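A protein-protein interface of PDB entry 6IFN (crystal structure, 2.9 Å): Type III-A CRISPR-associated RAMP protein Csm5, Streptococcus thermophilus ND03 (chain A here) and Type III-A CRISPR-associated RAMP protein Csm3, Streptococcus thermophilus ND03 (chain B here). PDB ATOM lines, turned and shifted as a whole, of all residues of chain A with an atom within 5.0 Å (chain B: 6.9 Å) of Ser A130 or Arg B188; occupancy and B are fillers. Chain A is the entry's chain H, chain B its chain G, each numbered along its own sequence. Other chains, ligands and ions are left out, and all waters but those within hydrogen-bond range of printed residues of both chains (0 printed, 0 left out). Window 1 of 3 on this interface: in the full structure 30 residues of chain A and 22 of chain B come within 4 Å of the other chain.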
ATOM      1  N   PRO A 128      14.712 -24.112  -8.623  1.00  0.00           N
ATOM      2  CA  PRO A 128      15.739 -23.323  -7.947  1.00  0.00           C
ATOM      3  C   PRO A 128      16.533 -22.483  -8.955  1.00  0.00           C
ATOM      4  O   PRO A 128      17.066 -22.997  -9.921  1.00  0.00           O
ATOM      5  CB  PRO A 128      16.626 -24.358  -7.239  1.00  0.00           C
ATOM      6  CG  PRO A 128      16.350 -25.667  -7.959  1.00  0.00           C
ATOM      7  CD  PRO A 128      14.926 -25.564  -8.467  1.00  0.00           C
ATOM      8  N   GLY A 129      16.616 -21.185  -8.686  1.00  0.00           N
ATOM      9  CA  GLY A 129      17.372 -20.265  -9.489  1.00  0.00           C
ATOM     10  C   GLY A 129      18.810 -20.717  -9.672  1.00  0.00           C
ATOM     11  O   GLY A 129      19.479 -20.279 -10.599  1.00  0.00           O
ATOM     12  N   SER A 130      19.294 -21.580  -8.777  1.00  0.00           N
ATOM     13  CA  SER A 130      20.630 -22.103  -8.898  1.00  0.00           C
ATOM     14  C   SER A 130      20.725 -22.934 -10.180  1.00  0.00           C
ATOM     15  O   SER A 130      21.715 -22.840 -10.923  1.00  0.00           O
ATOM     16  CB  SER A 130      21.018 -22.890  -7.680  1.00  0.00           C
ATOM     17  OG  SER A 130      20.155 -23.999  -7.499  1.00  0.00           O
ATOM     18  N   SER A 131      19.688 -23.731 -10.442  1.00  0.00           N
ATOM     19  CA  SER A 131      19.699 -24.615 -11.585  1.00  0.00           C
ATOM     20  C   SER A 131      19.506 -23.808 -12.875  1.00  0.00           C
ATOM     21  O   SER A 131      20.261 -23.997 -13.845  1.00  0.00           O
ATOM     22  CB  SER A 131      18.704 -25.739 -11.426  1.00  0.00           C
ATOM     23  OG  SER A 131      17.519 -25.268 -10.817  1.00  0.00           O
ATOM     24  N   LEU A 132      18.559 -22.866 -12.872  1.00  0.00           N
ATOM     25  CA  LEU A 132      18.402 -22.027 -14.051  1.00  0.00           C
ATOM     26  C   LEU A 132      19.717 -21.284 -14.330  1.00  0.00           C
ATOM     27  O   LEU A 132      20.122 -21.155 -15.484  1.00  0.00           O
ATOM     28  CB  LEU A 132      17.245 -21.040 -13.896  1.00  0.00           C
ATOM     29  CG  LEU A 132      16.993 -20.161 -15.129  1.00  0.00           C
ATOM     30  CD1 LEU A 132      15.516 -19.977 -15.401  1.00  0.00           C
ATOM     31  CD2 LEU A 132      17.622 -18.798 -14.990  1.00  0.00           C
ATOM     32  N   LYS A 133      20.383 -20.797 -13.278  1.00  0.00           N
ATOM     33  CA  LYS A 133      21.615 -20.021 -13.464  1.00  0.00           C
ATOM     34  C   LYS A 133      22.689 -20.907 -14.097  1.00  0.00           C
ATOM     35  O   LYS A 133      23.521 -20.432 -14.869  1.00  0.00           O
ATOM     36  CB  LYS A 133      22.168 -19.440 -12.158  1.00  0.00           C
ATOM     37  CG  LYS A 133      23.357 -18.505 -12.364  1.00  0.00           C
ATOM     38  CD  LYS A 133      24.089 -18.097 -11.108  1.00  0.00           C
ATOM     39  CE  LYS A 133      24.908 -16.841 -11.323  1.00  0.00           C
ATOM     40  NZ  LYS A 133      25.607 -16.417 -10.091  1.00  0.00           N
ATOM     41  N   GLY A 134      22.689 -22.186 -13.725  1.00  0.00           N
ATOM     42  CA  GLY A 134      23.589 -23.126 -14.337  1.00  0.00           C
ATOM     43  C   GLY A 134      23.465 -23.100 -15.848  1.00  0.00           C
ATOM     44  O   GLY A 134      24.462 -22.997 -16.569  1.00  0.00           O
ATOM     45  N   VAL A 186      19.957 -14.881  -9.973  1.00  0.00           N
ATOM     46  CA  VAL A 186      18.832 -15.627 -10.564  1.00  0.00           C
ATOM     47  C   VAL A 186      17.866 -16.059  -9.455  1.00  0.00           C
ATOM     48  O   VAL A 186      18.217 -16.915  -8.632  1.00  0.00           O
ATOM     49  CB  VAL A 186      19.327 -16.853 -11.364  1.00  0.00           C
ATOM     50  CG1 VAL A 186      18.191 -17.790 -11.718  1.00  0.00           C
ATOM     51  CG2 VAL A 186      20.086 -16.446 -12.621  1.00  0.00           C
ATOM     52  N   ASP A 188      15.073 -17.746  -7.210  1.00  0.00           N
ATOM     53  CA  ASP A 188      14.367 -18.997  -7.023  1.00  0.00           C
ATOM     54  C   ASP A 188      12.980 -18.787  -7.627  1.00  0.00           C
ATOM     55  O   ASP A 188      12.411 -17.676  -7.568  1.00  0.00           O
ATOM     56  CB  ASP A 188      14.281 -19.427  -5.552  1.00  0.00           C
ATOM     57  CG  ASP A 188      15.363 -20.387  -5.063  1.00  0.00           C
ATOM     58  OD1 ASP A 188      16.315 -20.692  -5.838  1.00  0.00           O
ATOM     59  OD2 ASP A 188      15.246 -20.842  -3.900  1.00  0.00           O
ATOM     60  N   LYS B 121      19.042 -27.872   1.197  1.00  0.00           N
ATOM     61  CA  LYS B 121      19.025 -27.842  -0.244  1.00  0.00           C
ATOM     62  C   LYS B 121      20.247 -28.601  -0.776  1.00  0.00           C
ATOM     63  O   LYS B 121      21.385 -28.305  -0.387  1.00  0.00           O
ATOM     64  CB  LYS B 121      19.028 -26.389  -0.721  1.00  0.00           C
ATOM     65  CG  LYS B 121      18.646 -26.165  -2.175  1.00  0.00           C
ATOM     66  CD  LYS B 121      18.664 -24.720  -2.551  1.00  0.00           C
ATOM     67  CE  LYS B 121      18.570 -24.486  -4.042  1.00  0.00           C
ATOM     68  NZ  LYS B 121      18.515 -23.037  -4.376  1.00  0.00           N
ATOM     69  N   PHE B 122      19.992 -29.547  -1.688  1.00  0.00           N
ATOM     70  CA  PHE B 122      21.037 -30.145  -2.510  1.00  0.00           C
ATOM     71  C   PHE B 122      21.250 -29.314  -3.786  1.00  0.00           C
ATOM     72  O   PHE B 122      20.287 -28.984  -4.497  1.00  0.00           O
ATOM     73  CB  PHE B 122      20.659 -31.585  -2.828  1.00  0.00           C
ATOM     74  CG  PHE B 122      20.962 -32.544  -1.710  1.00  0.00           C
ATOM     75  CD1 PHE B 122      20.222 -32.550  -0.541  1.00  0.00           C
ATOM     76  CD2 PHE B 122      21.977 -33.477  -1.850  1.00  0.00           C
ATOM     77  CE1 PHE B 122      20.494 -33.468   0.466  1.00  0.00           C
ATOM     78  CE2 PHE B 122      22.260 -34.387  -0.839  1.00  0.00           C
ATOM     79  CZ  PHE B 122      21.503 -34.391   0.309  1.00  0.00           C
ATOM     80  N   GLU B 123      22.520 -28.981  -4.032  1.00  0.00           N
ATOM     81  CA  GLU B 123      22.965 -28.342  -5.245  1.00  0.00           C
ATOM     82  C   GLU B 123      24.187 -29.109  -5.759  1.00  0.00           C
ATOM     83  O   GLU B 123      24.752 -29.937  -5.041  1.00  0.00           O
ATOM     84  CB  GLU B 123      23.300 -26.872  -4.987  1.00  0.00           C
ATOM     85  CG  GLU B 123      22.175 -26.126  -4.313  1.00  0.00           C
ATOM     86  CD  GLU B 123      22.492 -24.725  -3.816  1.00  0.00           C
ATOM     87  OE1 GLU B 123      21.782 -24.294  -2.920  1.00  0.00           O
ATOM     88  OE2 GLU B 123      23.426 -24.078  -4.312  1.00  0.00           O
ATOM     89  N   ASN B 124      24.609 -28.812  -6.986  1.00  0.00           N
ATOM     90  CA  ASN B 124      25.856 -29.317  -7.470  1.00  0.00           C
ATOM     91  C   ASN B 124      26.456 -28.319  -8.451  1.00  0.00           C
ATOM     92  O   ASN B 124      25.861 -27.276  -8.751  1.00  0.00           O
ATOM     93  CB  ASN B 124      25.704 -30.694  -8.113  1.00  0.00           C
ATOM     94  CG  ASN B 124      25.098 -30.679  -9.495  1.00  0.00           C
ATOM     95  OD1 ASN B 124      24.520 -29.684  -9.941  1.00  0.00           O
ATOM     96  ND2 ASN B 124      25.226 -31.813 -10.168  1.00  0.00           N
ATOM     97  N   ARG B 136      26.726 -30.763  -3.255  1.00  0.00           N
ATOM     98  CA  ARG B 136      26.882 -30.075  -2.034  1.00  0.00           C
ATOM     99  C   ARG B 136      25.513 -29.845  -1.407  1.00  0.00           C
ATOM    100  O   ARG B 136      24.560 -29.558  -2.090  1.00  0.00           O
ATOM    101  CB  ARG B 136      27.616 -28.761  -2.271  1.00  0.00           C
ATOM    102  CG  ARG B 136      26.747 -27.623  -2.765  1.00  0.00           C
ATOM    103  CD  ARG B 136      27.645 -26.567  -3.411  1.00  0.00           C
ATOM    104  NE  ARG B 136      26.971 -25.320  -3.754  1.00  0.00           N
ATOM    105  CZ  ARG B 136      26.626 -24.959  -4.991  1.00  0.00           C
ATOM    106  NH1 ARG B 136      27.000 -25.697  -6.025  1.00  0.00           N
ATOM    107  NH2 ARG B 136      25.873 -23.890  -5.187  1.00  0.00           N
ATOM    108  N   ILE B 138      23.389 -27.614   1.611  1.00  0.00           N
ATOM    109  CA  ILE B 138      23.448 -26.443   2.453  1.00  0.00           C
ATOM    110  C   ILE B 138      22.060 -26.182   3.059  1.00  0.00           C
ATOM    111  O   ILE B 138      21.051 -26.268   2.380  1.00  0.00           O
ATOM    112  CB  ILE B 138      23.989 -25.222   1.686  1.00  0.00           C
ATOM    113  CG1 ILE B 138      22.900 -24.501   0.896  1.00  0.00           C
ATOM    114  CG2 ILE B 138      25.172 -25.591   0.799  1.00  0.00           C
ATOM    115  CD1 ILE B 138      23.375 -23.212   0.304  1.00  0.00           C
ATOM    116  N   ARG B 140      19.134 -23.920   4.813  1.00  0.00           N
ATOM    117  CA  ARG B 140      18.477 -22.655   4.612  1.00  0.00           C
ATOM    118  C   ARG B 140      17.326 -22.582   5.611  1.00  0.00           C
ATOM    119  O   ARG B 140      16.728 -23.607   5.954  1.00  0.00           O
ATOM    120  CB  ARG B 140      17.880 -22.512   3.204  1.00  0.00           C
ATOM    121  CG  ARG B 140      18.741 -23.059   2.068  1.00  0.00           C
ATOM    122  CD  ARG B 140      17.940 -23.315   0.804  1.00  0.00           C
ATOM    123  NE  ARG B 140      17.641 -22.090   0.082  1.00  0.00           N
ATOM    124  CZ  ARG B 140      16.606 -21.939  -0.734  1.00  0.00           C
ATOM    125  NH1 ARG B 140      15.651 -22.855  -0.760  1.00  0.00           N
ATOM    126  NH2 ARG B 140      16.489 -20.832  -1.443  1.00  0.00           N
ATOM    127  N   GLY B 184      23.840 -14.545   2.056  1.00  0.00           N
ATOM    128  CA  GLY B 184      23.636 -15.964   1.833  1.00  0.00           C
ATOM    129  C   GLY B 184      24.284 -16.312   0.516  1.00  0.00           C
ATOM    130  O   GLY B 184      25.275 -15.711   0.169  1.00  0.00           O
ATOM    131  N   SER B 185      23.721 -17.250  -0.232  1.00  0.00           N
ATOM    132  CA  SER B 185      24.205 -17.438  -1.572  1.00  0.00           C
ATOM    133  C   SER B 185      23.285 -16.646  -2.490  1.00  0.00           C
ATOM    134  O   SER B 185      22.392 -17.192  -3.085  1.00  0.00           O
ATOM    135  CB  SER B 185      24.309 -18.892  -1.916  1.00  0.00           C
ATOM    136  OG  SER B 185      24.934 -19.561  -0.839  1.00  0.00           O
ATOM    137  N   GLY B 186      23.481 -15.328  -2.504  1.00  0.00           N
ATOM    138  CA  GLY B 186      22.481 -14.398  -3.001  1.00  0.00           C
ATOM    139  C   GLY B 186      22.375 -14.426  -4.510  1.00  0.00           C
ATOM    140  O   GLY B 186      21.267 -14.328  -5.044  1.00  0.00           O
ATOM    141  N   SER B 187      23.527 -14.567  -5.175  1.00  0.00           N
ATOM    142  CA  SER B 187      23.605 -14.601  -6.624  1.00  0.00           C
ATOM    143  C   SER B 187      22.829 -15.799  -7.178  1.00  0.00           C
ATOM    144  O   SER B 187      22.417 -15.774  -8.323  1.00  0.00           O
ATOM    145  CB  SER B 187      25.031 -14.605  -7.101  1.00  0.00           C
ATOM    146  OG  SER B 187      25.575 -15.912  -7.053  1.00  0.00           O
ATOM    147  N   ARG B 188      22.638 -16.832  -6.358  1.00  0.00           N
ATOM    148  CA  ARG B 188      21.913 -18.030  -6.751  1.00  0.00           C
ATOM    149  C   ARG B 188      20.505 -18.028  -6.135  1.00  0.00           C
ATOM    150  O   ARG B 188      19.881 -19.090  -6.001  1.00  0.00           O
ATOM    151  CB  ARG B 188      22.742 -19.254  -6.354  1.00  0.00           C
ATOM    152  CG  ARG B 188      24.035 -19.393  -7.138  1.00  0.00           C
ATOM    153  CD  ARG B 188      24.964 -20.466  -6.605  1.00  0.00           C
ATOM    154  NE  ARG B 188      25.580 -20.053  -5.358  1.00  0.00           N
ATOM    155  CZ  ARG B 188      26.574 -19.171  -5.257  1.00  0.00           C
ATOM    156  NH1 ARG B 188      27.152 -18.685  -6.343  1.00  0.00           N
ATOM    157  NH2 ARG B 188      26.978 -18.766  -4.070  1.00  0.00           N
ATOM    158  N   GLY B 189      20.034 -16.835  -5.732  1.00  0.00           N
ATOM    159  CA  GLY B 189      18.629 -16.543  -5.427  1.00  0.00           C
ATOM    160  C   GLY B 189      18.236 -16.633  -3.950  1.00  0.00           C
ATOM    161  O   GLY B 189      17.054 -16.709  -3.618  1.00  0.00           O
ATOM    162  N   TYR B 190      19.204 -16.559  -3.044  1.00  0.00           N
ATOM    163  CA  TYR B 190      18.909 -16.693  -1.630  1.00  0.00           C
ATOM    164  C   TYR B 190      18.522 -15.326  -1.079  1.00  0.00           C
ATOM    165  O   TYR B 190      18.634 -14.303  -1.769  1.00  0.00           O
ATOM    166  CB  TYR B 190      20.115 -17.201  -0.853  1.00  0.00           C
ATOM    167  CG  TYR B 190      20.388 -18.666  -1.006  1.00  0.00           C
ATOM    168  CD1 TYR B 190      20.260 -19.294  -2.227  1.00  0.00           C
ATOM    169  CD2 TYR B 190      20.811 -19.416   0.075  1.00  0.00           C
ATOM    170  CE1 TYR B 190      20.548 -20.640  -2.372  1.00  0.00           C
ATOM    171  CE2 TYR B 190      21.119 -20.756  -0.056  1.00  0.00           C
ATOM    172  CZ  TYR B 190      20.999 -21.366  -1.285  1.00  0.00           C
ATOM    173  OH  TYR B 190      21.273 -22.688  -1.416  1.00  0.00           O
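OD1 of Asp A188 is in salt-bridge range of NZ of Lys B121, at 3.5 Å. O of Val A186 lies close to N of Gly B189 (3.4 Å). N of Val A186 is in hydrogen-bond range of O of Ser B187 (3.1 Å). NH2 of Arg B140 is in salt-bridge range of OD2 of Asp A188, 2.8 Å away. OG of Ser B187 lies within hydrogen-bond range of NZ of Lys A133.
NZ of Lys B121 is in salt-bridge range of OE1 of Glu B123, at 3.8 Å. The backbone carbonyl oxygen of Ile B138 is in hydrogen-bond range of the backbone NH of Lys B121, 2.8 Å away. OG of Ser B187 sits at hydrogen-bond distance from NH1 of Arg B188 (3.3 Å). O of Pro A128 lies within hydrogen-bond range of OG of Ser A131, at 2.5 Å. The backbone NH (N) of Gly A129 lies within hydrogen-bond range of the side-chain carboxylate (OD1) of Asp A188 (2.9 Å).
Among the printed residues, pairs that only touch across the chains: Val A186 with Arg B188, Ser A130 with Lys B121, Pro A128 with Lys B121, Ser A130 with Arg B188 and Asp A188 with Arg B188.
No residue of chain B comes within 4 Å of Gly A129. Of the printed residues of chain B, Asp A188 touches Lys B121, Arg B140 and Arg B188. Of the printed residues of chain A, Ser B187 touches Lys A133 and Val A186. Of chain A, only Ser A130 (3.8 Å), Val A186 (3.6 Å) and Asp A188 (3.9 Å) come within 4 Å of Arg B188. The nearest printed residue of chain B that does not touch Val A186 is Gly B186 (5.1 Å).
Of the 9 printed residues of chain A, 5 touch a printed residue of chain B. Hydrophobic or aromatic side chains of chain A that line the printed part of chain B: Pro A128. Along chain A the printed residues that touch a printed residue of chain B span positions 128 to 188. Of the 14 printed residues of chain B, 5 touch a printed residue of chain A. Among the printed residues, Asp or Glu carboxylates within 4 Å of a Lys or Arg side-chain nitrogen of the other chain: Asp A188 with Lys B121 (3.5 Å) and Asp A188 with Arg B140 (2.8 Å).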
